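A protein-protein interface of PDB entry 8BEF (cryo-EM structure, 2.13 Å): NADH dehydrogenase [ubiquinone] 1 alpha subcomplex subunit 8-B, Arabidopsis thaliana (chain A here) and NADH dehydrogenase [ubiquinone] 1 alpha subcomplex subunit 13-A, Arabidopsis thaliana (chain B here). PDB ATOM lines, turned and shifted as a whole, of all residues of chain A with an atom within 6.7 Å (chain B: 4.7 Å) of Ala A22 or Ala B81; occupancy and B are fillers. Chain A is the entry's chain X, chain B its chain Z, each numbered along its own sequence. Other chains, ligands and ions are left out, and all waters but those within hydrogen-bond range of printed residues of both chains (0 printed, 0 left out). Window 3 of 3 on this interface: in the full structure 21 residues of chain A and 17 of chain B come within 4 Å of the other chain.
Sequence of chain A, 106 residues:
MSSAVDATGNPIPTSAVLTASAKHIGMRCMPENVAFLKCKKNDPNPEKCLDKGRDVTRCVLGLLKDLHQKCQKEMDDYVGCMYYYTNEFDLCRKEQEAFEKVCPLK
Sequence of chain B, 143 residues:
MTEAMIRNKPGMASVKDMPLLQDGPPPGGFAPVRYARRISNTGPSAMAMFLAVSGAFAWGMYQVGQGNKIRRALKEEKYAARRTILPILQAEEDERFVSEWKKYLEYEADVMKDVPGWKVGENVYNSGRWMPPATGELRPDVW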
ATOM      1  N   VAL A  17      11.087 -28.104 -15.594  1.00  0.00           N
ATOM      2  CA  VAL A  17      10.676 -29.497 -15.769  1.00  0.00           C
ATOM      3  C   VAL A  17       9.203 -29.666 -15.417  1.00  0.00           C
ATOM      4  O   VAL A  17       8.426 -30.262 -16.176  1.00  0.00           O
ATOM      5  CB  VAL A  17      11.567 -30.427 -14.925  1.00  0.00           C
ATOM      6  CG1 VAL A  17      10.975 -31.825 -14.878  1.00  0.00           C
ATOM      7  CG2 VAL A  17      12.985 -30.453 -15.484  1.00  0.00           C
ATOM      8  N   LEU A  18       8.794 -29.121 -14.270  1.00  0.00           N
ATOM      9  CA  LEU A  18       7.412 -29.264 -13.829  1.00  0.00           C
ATOM     10  C   LEU A  18       6.450 -28.569 -14.786  1.00  0.00           C
ATOM     11  O   LEU A  18       5.409 -29.126 -15.142  1.00  0.00           O
ATOM     12  CB  LEU A  18       7.257 -28.719 -12.411  1.00  0.00           C
ATOM     13  CG  LEU A  18       8.051 -29.481 -11.347  1.00  0.00           C
ATOM     14  CD1 LEU A  18       8.040 -28.742 -10.020  1.00  0.00           C
ATOM     15  CD2 LEU A  18       7.505 -30.889 -11.192  1.00  0.00           C
ATOM     16  N   THR A  19       6.781 -27.348 -15.212  1.00  0.00           N
ATOM     17  CA  THR A  19       5.896 -26.634 -16.126  1.00  0.00           C
ATOM     18  C   THR A  19       5.780 -27.360 -17.458  1.00  0.00           C
ATOM     19  O   THR A  19       4.679 -27.499 -18.000  1.00  0.00           O
ATOM     20  CB  THR A  19       6.378 -25.196 -16.329  1.00  0.00           C
ATOM     21  OG1 THR A  19       6.687 -24.610 -15.059  1.00  0.00           O
ATOM     22  CG2 THR A  19       5.291 -24.369 -16.995  1.00  0.00           C
ATOM     23  N   ALA A  20       6.900 -27.857 -17.990  1.00  0.00           N
ATOM     24  CA  ALA A  20       6.850 -28.598 -19.244  1.00  0.00           C
ATOM     25  C   ALA A  20       6.039 -29.882 -19.109  1.00  0.00           C
ATOM     26  O   ALA A  20       5.369 -30.291 -20.063  1.00  0.00           O
ATOM     27  CB  ALA A  20       8.265 -28.910 -19.731  1.00  0.00           C
ATOM     28  N   SER A  21       6.077 -30.523 -17.942  1.00  0.00           N
ATOM     29  CA  SER A  21       5.352 -31.771 -17.729  1.00  0.00           C
ATOM     30  C   SER A  21       3.962 -31.571 -17.135  1.00  0.00           C
ATOM     31  O   SER A  21       3.297 -32.565 -16.834  1.00  0.00           O
ATOM     32  CB  SER A  21       6.161 -32.696 -16.817  1.00  0.00           C
ATOM     33  OG  SER A  21       7.408 -33.025 -17.399  1.00  0.00           O
ATOM     34  N   ALA A  22       3.533 -30.320 -16.951  1.00  0.00           N
ATOM     35  CA  ALA A  22       2.302 -30.029 -16.218  1.00  0.00           C
ATOM     36  C   ALA A  22       1.085 -30.739 -16.803  1.00  0.00           C
ATOM     37  O   ALA A  22       0.217 -31.192 -16.053  1.00  0.00           O
ATOM     38  CB  ALA A  22       2.071 -28.520 -16.173  1.00  0.00           C
ATOM     39  N   LYS A  23       0.983 -30.826 -18.130  1.00  0.00           N
ATOM     40  CA  LYS A  23      -0.179 -31.484 -18.727  1.00  0.00           C
ATOM     41  C   LYS A  23      -0.209 -32.971 -18.375  1.00  0.00           C
ATOM     42  O   LYS A  23      -1.251 -33.507 -17.968  1.00  0.00           O
ATOM     43  CB  LYS A  23      -0.173 -31.279 -20.241  1.00  0.00           C
ATOM     44  CG  LYS A  23      -0.423 -29.836 -20.677  1.00  0.00           C
ATOM     45  CD  LYS A  23      -0.345 -29.693 -22.183  1.00  0.00           C
ATOM     46  CE  LYS A  23      -0.736 -28.298 -22.649  1.00  0.00           C
ATOM     47  NZ  LYS A  23       0.263 -27.255 -22.287  1.00  0.00           N
ATOM     48  N   HIS A  24       0.936 -33.646 -18.510  1.00  0.00           N
ATOM     49  CA  HIS A  24       1.038 -35.045 -18.104  1.00  0.00           C
ATOM     50  C   HIS A  24       0.735 -35.209 -16.622  1.00  0.00           C
ATOM     51  O   HIS A  24       0.085 -36.176 -16.216  1.00  0.00           O
ATOM     52  CB  HIS A  24       2.434 -35.581 -18.413  1.00  0.00           C
ATOM     53  CG  HIS A  24       2.721 -35.726 -19.873  1.00  0.00           C
ATOM     54  ND1 HIS A  24       3.370 -34.755 -20.604  1.00  0.00           N
ATOM     55  CD2 HIS A  24       2.463 -36.736 -20.737  1.00  0.00           C
ATOM     56  CE1 HIS A  24       3.490 -35.156 -21.857  1.00  0.00           C
ATOM     57  NE2 HIS A  24       2.950 -36.356 -21.963  1.00  0.00           N
ATOM     58  N   ILE A  25       1.216 -34.275 -15.799  1.00  0.00           N
ATOM     59  CA  ILE A  25       0.995 -34.353 -14.360  1.00  0.00           C
ATOM     60  C   ILE A  25      -0.490 -34.235 -14.044  1.00  0.00           C
ATOM     61  O   ILE A  25      -1.031 -34.993 -13.230  1.00  0.00           O
ATOM     62  CB  ILE A  25       1.821 -33.270 -13.640  1.00  0.00           C
ATOM     63  CG1 ILE A  25       3.315 -33.581 -13.742  1.00  0.00           C
ATOM     64  CG2 ILE A  25       1.398 -33.146 -12.190  1.00  0.00           C
ATOM     65  CD1 ILE A  25       4.200 -32.599 -13.011  1.00  0.00           C
ATOM     66  N   GLY A  26      -1.171 -33.287 -14.685  1.00  0.00           N
ATOM     67  CA  GLY A  26      -2.594 -33.123 -14.453  1.00  0.00           C
ATOM     68  C   GLY A  26      -3.394 -34.333 -14.887  1.00  0.00           C
ATOM     69  O   GLY A  26      -4.342 -34.736 -14.211  1.00  0.00           O
ATOM     70  N   MET A  27      -3.021 -34.934 -16.018  1.00  0.00           N
ATOM     71  CA  MET A  27      -3.723 -36.131 -16.462  1.00  0.00           C
ATOM     72  C   MET A  27      -3.409 -37.361 -15.615  1.00  0.00           C
ATOM     73  O   MET A  27      -4.257 -38.253 -15.508  1.00  0.00           O
ATOM     74  CB  MET A  27      -3.400 -36.423 -17.930  1.00  0.00           C
ATOM     75  CG  MET A  27      -4.340 -35.792 -18.973  1.00  0.00           C
ATOM     76  SD  MET A  27      -6.155 -35.738 -18.808  1.00  0.00           S
ATOM     77  CE  MET A  27      -6.582 -37.112 -17.732  1.00  0.00           C
ATOM     78  N   PHE A  89       4.772 -20.920 -22.959  1.00  0.00           N
ATOM     79  CA  PHE A  89       4.386 -22.018 -23.842  1.00  0.00           C
ATOM     80  C   PHE A  89       4.439 -21.612 -25.311  1.00  0.00           C
ATOM     81  O   PHE A  89       4.822 -22.415 -26.168  1.00  0.00           O
ATOM     82  CB  PHE A  89       2.985 -22.515 -23.482  1.00  0.00           C
ATOM     83  CG  PHE A  89       2.918 -23.260 -22.177  1.00  0.00           C
ATOM     84  CD1 PHE A  89       3.448 -24.536 -22.066  1.00  0.00           C
ATOM     85  CD2 PHE A  89       2.323 -22.688 -21.068  1.00  0.00           C
ATOM     86  CE1 PHE A  89       3.386 -25.228 -20.870  1.00  0.00           C
ATOM     87  CE2 PHE A  89       2.260 -23.378 -19.868  1.00  0.00           C
ATOM     88  CZ  PHE A  89       2.796 -24.648 -19.772  1.00  0.00           C
ATOM     89  N   LEU A 105      -0.089 -37.699 -24.212  1.00  0.00           N
ATOM     90  CA  LEU A 105      -0.765 -37.348 -22.966  1.00  0.00           C
ATOM     91  C   LEU A 105      -1.622 -38.499 -22.457  1.00  0.00           C
ATOM     92  O   LEU A 105      -1.681 -38.744 -21.248  1.00  0.00           O
ATOM     93  CB  LEU A 105      -1.612 -36.093 -23.168  1.00  0.00           C
ATOM     94  CG  LEU A 105      -0.814 -34.793 -23.275  1.00  0.00           C
ATOM     95  CD1 LEU A 105      -1.718 -33.621 -23.625  1.00  0.00           C
ATOM     96  CD2 LEU A 105      -0.064 -34.533 -21.984  1.00  0.00           C
ATOM     97  N   GLU B  77      -4.282 -21.576 -20.699  1.00  0.00           N
ATOM     98  CA  GLU B  77      -3.311 -22.661 -20.808  1.00  0.00           C
ATOM     99  C   GLU B  77      -2.221 -22.519 -19.753  1.00  0.00           C
ATOM    100  O   GLU B  77      -1.927 -23.466 -19.004  1.00  0.00           O
ATOM    101  CB  GLU B  77      -2.692 -22.696 -22.203  1.00  0.00           C
ATOM    102  CG  GLU B  77      -1.488 -23.618 -22.278  1.00  0.00           C
ATOM    103  CD  GLU B  77      -0.744 -23.543 -23.593  1.00  0.00           C
ATOM    104  OE1 GLU B  77      -1.057 -22.656 -24.414  1.00  0.00           O
ATOM    105  OE2 GLU B  77       0.164 -24.372 -23.800  1.00  0.00           O
ATOM    106  N   LYS B  78      -1.629 -21.325 -19.660  1.00  0.00           N
ATOM    107  CA  LYS B  78      -0.615 -21.106 -18.627  1.00  0.00           C
ATOM    108  C   LYS B  78      -1.187 -21.348 -17.232  1.00  0.00           C
ATOM    109  O   LYS B  78      -0.522 -21.928 -16.361  1.00  0.00           O
ATOM    110  CB  LYS B  78      -0.040 -19.694 -18.735  1.00  0.00           C
ATOM    111  CG  LYS B  78       0.927 -19.334 -17.621  1.00  0.00           C
ATOM    112  CD  LYS B  78       1.435 -17.914 -17.767  1.00  0.00           C
ATOM    113  CE  LYS B  78       0.816 -17.000 -16.739  1.00  0.00           C
ATOM    114  NZ  LYS B  78      -0.569 -16.648 -17.145  1.00  0.00           N
ATOM    115  N   TYR B  79      -2.433 -20.937 -17.018  1.00  0.00           N
ATOM    116  CA  TYR B  79      -2.994 -20.933 -15.675  1.00  0.00           C
ATOM    117  C   TYR B  79      -3.350 -22.355 -15.248  1.00  0.00           C
ATOM    118  O   TYR B  79      -3.205 -22.719 -14.076  1.00  0.00           O
ATOM    119  CB  TYR B  79      -4.218 -20.020 -15.670  1.00  0.00           C
ATOM    120  CG  TYR B  79      -3.833 -18.571 -15.507  1.00  0.00           C
ATOM    121  CD1 TYR B  79      -2.769 -18.195 -14.704  1.00  0.00           C
ATOM    122  CD2 TYR B  79      -4.454 -17.593 -16.272  1.00  0.00           C
ATOM    123  CE1 TYR B  79      -2.389 -16.877 -14.601  1.00  0.00           C
ATOM    124  CE2 TYR B  79      -4.066 -16.279 -16.195  1.00  0.00           C
ATOM    125  CZ  TYR B  79      -3.037 -15.922 -15.350  1.00  0.00           C
ATOM    126  OH  TYR B  79      -2.651 -14.604 -15.252  1.00  0.00           O
ATOM    127  N   ALA B  80      -3.808 -23.173 -16.201  1.00  0.00           N
ATOM    128  CA  ALA B  80      -4.006 -24.594 -15.952  1.00  0.00           C
ATOM    129  C   ALA B  80      -2.684 -25.281 -15.654  1.00  0.00           C
ATOM    130  O   ALA B  80      -2.609 -26.133 -14.763  1.00  0.00           O
ATOM    131  CB  ALA B  80      -4.691 -25.248 -17.152  1.00  0.00           C
ATOM    132  N   ALA B  81      -1.627 -24.924 -16.390  1.00  0.00           N
ATOM    133  CA  ALA B  81      -0.318 -25.496 -16.093  1.00  0.00           C
ATOM    134  C   ALA B  81       0.097 -25.196 -14.659  1.00  0.00           C
ATOM    135  O   ALA B  81       0.604 -26.075 -13.956  1.00  0.00           O
ATOM    136  CB  ALA B  81       0.728 -24.970 -17.073  1.00  0.00           C
ATOM    137  N   ARG B  82      -0.127 -23.963 -14.201  1.00  0.00           N
ATOM    138  CA  ARG B  82       0.199 -23.645 -12.815  1.00  0.00           C
ATOM    139  C   ARG B  82      -0.660 -24.434 -11.835  1.00  0.00           C
ATOM    140  O   ARG B  82      -0.214 -24.739 -10.724  1.00  0.00           O
ATOM    141  CB  ARG B  82       0.050 -22.147 -12.568  1.00  0.00           C
ATOM    142  CG  ARG B  82       1.180 -21.333 -13.153  1.00  0.00           C
ATOM    143  CD  ARG B  82       0.848 -19.863 -13.176  1.00  0.00           C
ATOM    144  NE  ARG B  82       1.934 -19.079 -13.746  1.00  0.00           N
ATOM    145  CZ  ARG B  82       2.093 -17.777 -13.558  1.00  0.00           C
ATOM    146  NH1 ARG B  82       1.233 -17.073 -12.838  1.00  0.00           N
ATOM    147  NH2 ARG B  82       3.143 -17.168 -14.099  1.00  0.00           N
ATOM    148  N   ARG B  83      -1.887 -24.777 -12.226  1.00  0.00           N
ATOM    149  CA  ARG B  83      -2.791 -25.457 -11.306  1.00  0.00           C
ATOM    150  C   ARG B  83      -2.401 -26.917 -11.088  1.00  0.00           C
ATOM    151  O   ARG B  83      -2.564 -27.435  -9.979  1.00  0.00           O
ATOM    152  CB  ARG B  83      -4.227 -25.344 -11.821  1.00  0.00           C
ATOM    153  CG  ARG B  83      -4.960 -24.123 -11.287  1.00  0.00           C
ATOM    154  CD  ARG B  83      -6.451 -24.174 -11.575  1.00  0.00           C
ATOM    155  NE  ARG B  83      -6.718 -24.135 -13.007  1.00  0.00           N
ATOM    156  CZ  ARG B  83      -7.001 -23.034 -13.689  1.00  0.00           C
ATOM    157  NH1 ARG B  83      -7.113 -21.861 -13.091  1.00  0.00           N
ATOM    158  NH2 ARG B  83      -7.173 -23.113 -15.005  1.00  0.00           N
ATOM    159  N   THR B  84      -1.878 -27.592 -12.116  1.00  0.00           N
ATOM    160  CA  THR B  84      -1.561 -29.012 -11.973  1.00  0.00           C
ATOM    161  C   THR B  84      -0.300 -29.251 -11.150  1.00  0.00           C
ATOM    162  O   THR B  84      -0.186 -30.291 -10.495  1.00  0.00           O
ATOM    163  CB  THR B  84      -1.423 -29.685 -13.340  1.00  0.00           C
ATOM    164  OG1 THR B  84      -0.105 -29.470 -13.859  1.00  0.00           O
ATOM    165  CG2 THR B  84      -2.453 -29.163 -14.313  1.00  0.00           C
ATOM    166  N   ILE B  85       0.658 -28.320 -11.169  1.00  0.00           N
ATOM    167  CA  ILE B  85       1.878 -28.474 -10.381  1.00  0.00           C
ATOM    168  C   ILE B  85       1.800 -27.762  -9.041  1.00  0.00           C
ATOM    169  O   ILE B  85       2.770 -27.795  -8.273  1.00  0.00           O
ATOM    170  CB  ILE B  85       3.118 -28.000 -11.164  1.00  0.00           C
ATOM    171  CG1 ILE B  85       3.076 -26.486 -11.391  1.00  0.00           C
ATOM    172  CG2 ILE B  85       3.239 -28.752 -12.475  1.00  0.00           C
ATOM    173  CD1 ILE B  85       4.415 -25.886 -11.728  1.00  0.00           C
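Leu A18 touches Ile B85. O of Ala B81 touches CB of Ala A22, 3.6 Å away. Ile B85 touches Ala A22. Ile A25 touches Thr B84. CA of Gly A26 touches CB of Thr B84, 3.8 Å away. CG of Phe A89 touches OE2 of Glu B77 (3.4 Å). Phe A89 touches Lys B78. Phe A89 touches Ala B81 (CZ to CB, 3.4 Å).
Of the 9 printed residues of chain B, 5 touch a printed residue of chain A. Hydrophobic or aromatic side chains of chain B that line the printed part of chain A: Ala B81 and Ile B85. Along chain B the printed residues that touch a printed residue of chain A span positions 77 to 85. Hydrophobic or aromatic side chains of chain A that line the printed part of chain B: Ala A22, Ile A25 and Phe A89. Among the printed residues, 10 pairs touch across the chains.
The side-chain carboxylate (OE2) of Glu B77 lies within salt-bridge range of the side-chain amino group (NZ) of Lys A23 (3.3 Å). OG1 of Thr B84 lies within hydrogen-bond range of O of Ala A22, 2.8 Å away.
NZ of Lys B78 sits close to OH of Tyr B79 (3.5 Å). OG1 of Thr B84 is in hydrogen-bond range of O of Ala B81 (3.5 Å).
Of the printed residues of chain B, Ala A22 touches Ala B81 (3.6 Å), Thr B84 (2.8 Å) and Ile B85 (3.9 Å). Of chain A, only Ala A22 (3.6 Å) and Phe A89 (3.4 Å) come within 4 Å of Ala B81. Of the printed residues of chain A, Glu B77 touches Lys A23 (3.3 Å) and Phe A89 (3.4 Å). Printed residues of chain B within 4 Å of Ile A25: Thr B84. Printed residues of chain A within 4 Å of Ile B85: Leu A18 (3.5 Å) and Ala A22 (3.9 Å). Ala B80 touches none of the printed residues of chain A. The nearest residue of chain A that does not touch Ala B81 is Thr A19 (4.6 Å).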
